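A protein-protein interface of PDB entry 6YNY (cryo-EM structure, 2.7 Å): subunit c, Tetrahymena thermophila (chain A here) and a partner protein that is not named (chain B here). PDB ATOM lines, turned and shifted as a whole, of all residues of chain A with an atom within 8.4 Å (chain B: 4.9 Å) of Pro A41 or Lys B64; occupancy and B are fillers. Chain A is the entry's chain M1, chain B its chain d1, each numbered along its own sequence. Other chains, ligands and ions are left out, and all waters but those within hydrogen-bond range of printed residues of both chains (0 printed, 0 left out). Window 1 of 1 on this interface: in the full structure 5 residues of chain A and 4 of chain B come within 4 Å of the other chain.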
ATOM      1  N   PHE A  33       7.354  29.357 -16.387  1.00  0.00           N
ATOM      2  CA  PHE A  33       7.855  30.122 -15.251  1.00  0.00           C
ATOM      3  C   PHE A  33       7.814  29.295 -13.973  1.00  0.00           C
ATOM      4  O   PHE A  33       8.774  29.301 -13.194  1.00  0.00           O
ATOM      5  CB  PHE A  33       7.041  31.404 -15.092  1.00  0.00           C
ATOM      6  CG  PHE A  33       7.330  32.159 -13.828  1.00  0.00           C
ATOM      7  CD1 PHE A  33       6.348  32.328 -12.867  1.00  0.00           C
ATOM      8  CD2 PHE A  33       8.582  32.703 -13.599  1.00  0.00           C
ATOM      9  CE1 PHE A  33       6.610  33.024 -11.705  1.00  0.00           C
ATOM     10  CE2 PHE A  33       8.849  33.399 -12.436  1.00  0.00           C
ATOM     11  CZ  PHE A  33       7.860  33.560 -11.489  1.00  0.00           C
ATOM     12  N   ASN A  34       6.716  28.573 -13.742  1.00  0.00           N
ATOM     13  CA  ASN A  34       6.622  27.730 -12.554  1.00  0.00           C
ATOM     14  C   ASN A  34       7.746  26.701 -12.521  1.00  0.00           C
ATOM     15  O   ASN A  34       8.419  26.533 -11.497  1.00  0.00           O
ATOM     16  CB  ASN A  34       5.261  27.037 -12.513  1.00  0.00           C
ATOM     17  CG  ASN A  34       4.135  27.989 -12.180  1.00  0.00           C
ATOM     18  OD1 ASN A  34       4.253  29.199 -12.367  1.00  0.00           O
ATOM     19  ND2 ASN A  34       3.035  27.446 -11.679  1.00  0.00           N
ATOM     20  N   VAL A  35       7.963  26.000 -13.633  1.00  0.00           N
ATOM     21  CA  VAL A  35       9.035  25.011 -13.685  1.00  0.00           C
ATOM     22  C   VAL A  35      10.389  25.693 -13.555  1.00  0.00           C
ATOM     23  O   VAL A  35      11.177  25.380 -12.656  1.00  0.00           O
ATOM     24  CB  VAL A  35       8.940  24.185 -14.979  1.00  0.00           C
ATOM     25  CG1 VAL A  35      10.234  23.433 -15.223  1.00  0.00           C
ATOM     26  CG2 VAL A  35       7.772  23.219 -14.896  1.00  0.00           C
ATOM     27  N   ALA A  36      10.678  26.640 -14.450  1.00  0.00           N
ATOM     28  CA  ALA A  36      11.952  27.346 -14.394  1.00  0.00           C
ATOM     29  C   ALA A  36      12.201  27.930 -13.011  1.00  0.00           C
ATOM     30  O   ALA A  36      13.355  28.061 -12.586  1.00  0.00           O
ATOM     31  CB  ALA A  36      11.988  28.450 -15.450  1.00  0.00           C
ATOM     32  N   LEU A  37      11.133  28.286 -12.296  1.00  0.00           N
ATOM     33  CA  LEU A  37      11.285  28.843 -10.956  1.00  0.00           C
ATOM     34  C   LEU A  37      11.695  27.767  -9.957  1.00  0.00           C
ATOM     35  O   LEU A  37      12.620  27.965  -9.161  1.00  0.00           O
ATOM     36  CB  LEU A  37       9.978  29.509 -10.525  1.00  0.00           C
ATOM     37  CG  LEU A  37       9.953  30.197  -9.162  1.00  0.00           C
ATOM     38  CD1 LEU A  37      10.924  31.359  -9.118  1.00  0.00           C
ATOM     39  CD2 LEU A  37       8.542  30.668  -8.849  1.00  0.00           C
ATOM     40  N   SER A  38      11.017  26.617  -9.985  1.00  0.00           N
ATOM     41  CA  SER A  38      11.359  25.545  -9.056  1.00  0.00           C
ATOM     42  C   SER A  38      12.775  25.037  -9.286  1.00  0.00           C
ATOM     43  O   SER A  38      13.438  24.598  -8.340  1.00  0.00           O
ATOM     44  CB  SER A  38      10.357  24.397  -9.187  1.00  0.00           C
ATOM     45  OG  SER A  38      10.357  23.866 -10.499  1.00  0.00           O
ATOM     46  N   ARG A  39      13.255  25.088 -10.529  1.00  0.00           N
ATOM     47  CA  ARG A  39      14.617  24.649 -10.815  1.00  0.00           C
ATOM     48  C   ARG A  39      15.636  25.571 -10.159  1.00  0.00           C
ATOM     49  O   ARG A  39      16.570  25.109  -9.493  1.00  0.00           O
ATOM     50  CB  ARG A  39      14.840  24.594 -12.326  1.00  0.00           C
ATOM     51  CG  ARG A  39      13.885  23.664 -13.057  1.00  0.00           C
ATOM     52  CD  ARG A  39      14.127  22.205 -12.722  1.00  0.00           C
ATOM     53  NE  ARG A  39      13.233  21.329 -13.475  1.00  0.00           N
ATOM     54  CZ  ARG A  39      13.295  20.002 -13.465  1.00  0.00           C
ATOM     55  NH1 ARG A  39      14.214  19.380 -12.737  1.00  0.00           N
ATOM     56  NH2 ARG A  39      12.436  19.294 -14.183  1.00  0.00           N
ATOM     57  N   ASN A  40      15.473  26.881 -10.335  1.00  0.00           N
ATOM     58  CA  ASN A  40      16.387  27.876  -9.773  1.00  0.00           C
ATOM     59  C   ASN A  40      15.574  29.058  -9.271  1.00  0.00           C
ATOM     60  O   ASN A  40      15.478  30.098  -9.934  1.00  0.00           O
ATOM     61  CB  ASN A  40      17.418  28.318 -10.812  1.00  0.00           C
ATOM     62  CG  ASN A  40      18.326  29.415 -10.300  1.00  0.00           C
ATOM     63  OD1 ASN A  40      18.465  29.608  -9.093  1.00  0.00           O
ATOM     64  ND2 ASN A  40      18.949  30.141 -11.218  1.00  0.00           N
ATOM     65  N   PRO A  41      14.974  28.938  -8.083  1.00  0.00           N
ATOM     66  CA  PRO A  41      14.107  30.015  -7.580  1.00  0.00           C
ATOM     67  C   PRO A  41      14.860  31.236  -7.080  1.00  0.00           C
ATOM     68  O   PRO A  41      14.218  32.246  -6.769  1.00  0.00           O
ATOM     69  CB  PRO A  41      13.332  29.339  -6.446  1.00  0.00           C
ATOM     70  CG  PRO A  41      14.219  28.241  -5.984  1.00  0.00           C
ATOM     71  CD  PRO A  41      14.966  27.762  -7.196  1.00  0.00           C
ATOM     72  N   GLU A  42      16.190  31.177  -6.988  1.00  0.00           N
ATOM     73  CA  GLU A  42      16.943  32.310  -6.459  1.00  0.00           C
ATOM     74  C   GLU A  42      16.708  33.577  -7.272  1.00  0.00           C
ATOM     75  O   GLU A  42      16.798  34.685  -6.730  1.00  0.00           O
ATOM     76  CB  GLU A  42      18.434  31.980  -6.428  1.00  0.00           C
ATOM     77  CG  GLU A  42      19.316  33.128  -5.957  1.00  0.00           C
ATOM     78  CD  GLU A  42      20.760  32.715  -5.766  1.00  0.00           C
ATOM     79  OE1 GLU A  42      21.036  31.497  -5.748  1.00  0.00           O
ATOM     80  OE2 GLU A  42      21.622  33.610  -5.633  1.00  0.00           O
ATOM     81  N   GLU A  43      16.407  33.438  -8.559  1.00  0.00           N
ATOM     82  CA  GLU A  43      16.219  34.572  -9.459  1.00  0.00           C
ATOM     83  C   GLU A  43      14.757  34.724  -9.871  1.00  0.00           C
ATOM     84  O   GLU A  43      14.450  35.046 -11.021  1.00  0.00           O
ATOM     85  CB  GLU A  43      17.112  34.432 -10.688  1.00  0.00           C
ATOM     86  CG  GLU A  43      16.913  33.143 -11.453  1.00  0.00           C
ATOM     87  CD  GLU A  43      17.771  33.072 -12.697  1.00  0.00           C
ATOM     88  OE1 GLU A  43      18.571  34.005 -12.921  1.00  0.00           O
ATOM     89  OE2 GLU A  43      17.646  32.084 -13.449  1.00  0.00           O
ATOM     90  N   THR A  44      13.840  34.486  -8.930  1.00  0.00           N
ATOM     91  CA  THR A  44      12.417  34.623  -9.228  1.00  0.00           C
ATOM     92  C   THR A  44      12.109  35.985  -9.834  1.00  0.00           C
ATOM     93  O   THR A  44      11.309  36.092 -10.769  1.00  0.00           O
ATOM     94  CB  THR A  44      11.588  34.408  -7.960  1.00  0.00           C
ATOM     95  OG1 THR A  44      10.193  34.459  -8.284  1.00  0.00           O
ATOM     96  CG2 THR A  44      11.892  35.476  -6.922  1.00  0.00           C
ATOM     97  N   GLU A  45      12.736  37.041  -9.311  1.00  0.00           N
ATOM     98  CA  GLU A  45      12.485  38.382  -9.827  1.00  0.00           C
ATOM     99  C   GLU A  45      12.823  38.472 -11.310  1.00  0.00           C
ATOM    100  O   GLU A  45      12.071  39.072 -12.089  1.00  0.00           O
ATOM    101  CB  GLU A  45      13.277  39.415  -9.023  1.00  0.00           C
ATOM    102  CG  GLU A  45      14.780  39.461  -9.302  1.00  0.00           C
ATOM    103  CD  GLU A  45      15.493  38.170  -8.950  1.00  0.00           C
ATOM    104  OE1 GLU A  45      14.866  37.294  -8.320  1.00  0.00           O
ATOM    105  OE2 GLU A  45      16.682  38.031  -9.307  1.00  0.00           O
ATOM    106  N   SER A  46      13.945  37.883 -11.724  1.00  0.00           N
ATOM    107  CA  SER A  46      14.318  37.914 -13.133  1.00  0.00           C
ATOM    108  C   SER A  46      13.293  37.165 -13.976  1.00  0.00           C
ATOM    109  O   SER A  46      12.733  37.712 -14.933  1.00  0.00           O
ATOM    110  CB  SER A  46      15.715  37.318 -13.315  1.00  0.00           C
ATOM    111  OG  SER A  46      16.122  37.378 -14.671  1.00  0.00           O
ATOM    112  N   LEU A  47      13.037  35.900 -13.633  1.00  0.00           N
ATOM    113  CA  LEU A  47      12.039  35.124 -14.361  1.00  0.00           C
ATOM    114  C   LEU A  47      10.680  35.811 -14.320  1.00  0.00           C
ATOM    115  O   LEU A  47      10.014  35.963 -15.350  1.00  0.00           O
ATOM    116  CB  LEU A  47      11.948  33.715 -13.772  1.00  0.00           C
ATOM    117  CG  LEU A  47      13.228  32.876 -13.778  1.00  0.00           C
ATOM    118  CD1 LEU A  47      13.047  31.626 -12.932  1.00  0.00           C
ATOM    119  CD2 LEU A  47      13.630  32.501 -15.191  1.00  0.00           C
ATOM    120  N   GLN B  62      23.536  27.384  -7.215  1.00  0.00           N
ATOM    121  CA  GLN B  62      23.632  28.591  -6.406  1.00  0.00           C
ATOM    122  C   GLN B  62      22.681  28.445  -5.224  1.00  0.00           C
ATOM    123  O   GLN B  62      22.164  27.359  -4.944  1.00  0.00           O
ATOM    124  CB  GLN B  62      23.325  29.833  -7.251  1.00  0.00           C
ATOM    125  CG  GLN B  62      21.969  29.788  -7.939  1.00  0.00           C
ATOM    126  CD  GLN B  62      21.614  31.078  -8.666  1.00  0.00           C
ATOM    127  OE1 GLN B  62      20.447  31.325  -8.965  1.00  0.00           O
ATOM    128  NE2 GLN B  62      22.617  31.899  -8.961  1.00  0.00           N
ATOM    129  N   ASN B  63      22.450  29.553  -4.525  1.00  0.00           N
ATOM    130  CA  ASN B  63      21.596  29.530  -3.347  1.00  0.00           C
ATOM    131  C   ASN B  63      20.187  29.074  -3.707  1.00  0.00           C
ATOM    132  O   ASN B  63      19.678  29.347  -4.797  1.00  0.00           O
ATOM    133  CB  ASN B  63      21.555  30.914  -2.699  1.00  0.00           C
ATOM    134  CG  ASN B  63      20.720  30.939  -1.439  1.00  0.00           C
ATOM    135  OD1 ASN B  63      19.737  31.674  -1.344  1.00  0.00           O
ATOM    136  ND2 ASN B  63      21.101  30.124  -0.464  1.00  0.00           N
ATOM    137  N   LYS B  64      19.565  28.356  -2.774  1.00  0.00           N
ATOM    138  CA  LYS B  64      18.208  27.828  -2.887  1.00  0.00           C
ATOM    139  C   LYS B  64      18.071  26.761  -3.962  1.00  0.00           C
ATOM    140  O   LYS B  64      16.944  26.361  -4.282  1.00  0.00           O
ATOM    141  CB  LYS B  64      17.190  28.940  -3.163  1.00  0.00           C
ATOM    142  CG  LYS B  64      16.968  29.883  -1.995  1.00  0.00           C
ATOM    143  CD  LYS B  64      16.063  31.050  -2.370  1.00  0.00           C
ATOM    144  CE  LYS B  64      14.674  30.590  -2.794  1.00  0.00           C
ATOM    145  NZ  LYS B  64      14.013  29.752  -1.757  1.00  0.00           N
ATOM    146  N   THR B  65      19.171  26.287  -4.531  1.00  0.00           N
ATOM    147  CA  THR B  65      19.081  25.235  -5.531  1.00  0.00           C
ATOM    148  C   THR B  65      18.464  23.990  -4.895  1.00  0.00           C
ATOM    149  O   THR B  65      18.936  23.545  -3.839  1.00  0.00           O
ATOM    150  CB  THR B  65      20.459  24.912  -6.102  1.00  0.00           C
ATOM    151  OG1 THR B  65      21.045  26.102  -6.642  1.00  0.00           O
ATOM    152  CG2 THR B  65      20.346  23.875  -7.200  1.00  0.00           C
ATOM    153  N   PRO B  66      17.422  23.406  -5.486  1.00  0.00           N
ATOM    154  CA  PRO B  66      16.782  22.241  -4.862  1.00  0.00           C
ATOM    155  C   PRO B  66      17.758  21.090  -4.679  1.00  0.00           C
ATOM    156  O   PRO B  66      18.867  21.069  -5.216  1.00  0.00           O
ATOM    157  CB  PRO B  66      15.664  21.874  -5.843  1.00  0.00           C
ATOM    158  CG  PRO B  66      15.404  23.115  -6.609  1.00  0.00           C
ATOM    159  CD  PRO B  66      16.722  23.816  -6.716  1.00  0.00           C
ATOM    160  N   ASN B 105      19.579  22.945   1.966  1.00  0.00           N
ATOM    161  CA  ASN B 105      20.213  23.980   1.150  1.00  0.00           C
ATOM    162  C   ASN B 105      21.730  23.977   1.342  1.00  0.00           C
ATOM    163  O   ASN B 105      22.344  24.972   1.726  1.00  0.00           O
ATOM    164  CB  ASN B 105      19.621  25.350   1.467  1.00  0.00           C
ATOM    165  CG  ASN B 105      19.996  26.400   0.442  1.00  0.00           C
ATOM    166  OD1 ASN B 105      20.676  26.109  -0.542  1.00  0.00           O
ATOM    167  ND2 ASN B 105      19.543  27.628   0.661  1.00  0.00           N
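The side-chain amide oxygen of Gln B62 lies close to the side-chain amide oxygen of Asn A40, 2.6 Å away.
The side-chain carboxylate of Glu A42 sits close to the side-chain amide oxygen of Gln B62.
The side-chain carboxylate (OE1) of Glu A42 sits at hydrogen-bond distance from the backbone NH (N) of Asn B63 (2.7 Å).
ND2 of Asn B63 sits close to ND2 of Asn B105, 3.2 Å away.
N of Gln B62 sits at hydrogen-bond distance from OG1 of Thr B65 (2.9 Å).
The backbone NH of Lys B64 is in hydrogen-bond range of the side-chain amide oxygen of Asn B105.
OD1 of Asn A40 sits close to N of Glu A42 (3.5 Å).
The side-chain hydroxyl of Ser A38 is in hydrogen-bond range of the backbone carbonyl oxygen of Asn A34 (3.4 Å).
The side-chain amide nitrogen (ND2) of Asn A40 sits at hydrogen-bond distance from the side-chain carboxylate (OE2) of Glu A43, 3.2 Å away.
Among the printed residues, merely in contact across the chains: Ser A38 with Pro B66, Arg A39 with Pro B66 and Pro A41 with Lys B64.
Of the printed residues of chain B, Arg A39 touches Pro B66 (3.1 Å).
Printed residues of chain B within 4 Å of Glu A42: Gln B62 and Asn B63.
Glu A45 touches none of the printed residues of chain B.
Printed residues of chain A within 4 Å of Gln B62: Asn A40 (2.6 Å) and Glu A42 (2.9 Å).
Asn B63 touches one residue of chain A.
Printed residues of chain A within 4 Å of Lys B64: Pro A41.
The nearest residue of chain B that does not touch Pro A41 is Pro B66 (4.3 Å).
The nearest residue of chain A that does not touch Lys B64 is Glu A42 (4.4 Å).
The nearest printed residue of chain B that does not touch Arg A39 is Thr B65 (4.6 Å).
Printed residues of chain B that touch a printed residue of chain A: Gln B62, Asn B63, Lys B64 and Pro B66.
Hydrophobic or aromatic side chains of chain B within 4 Å of the printed part of chain A: Pro B66.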
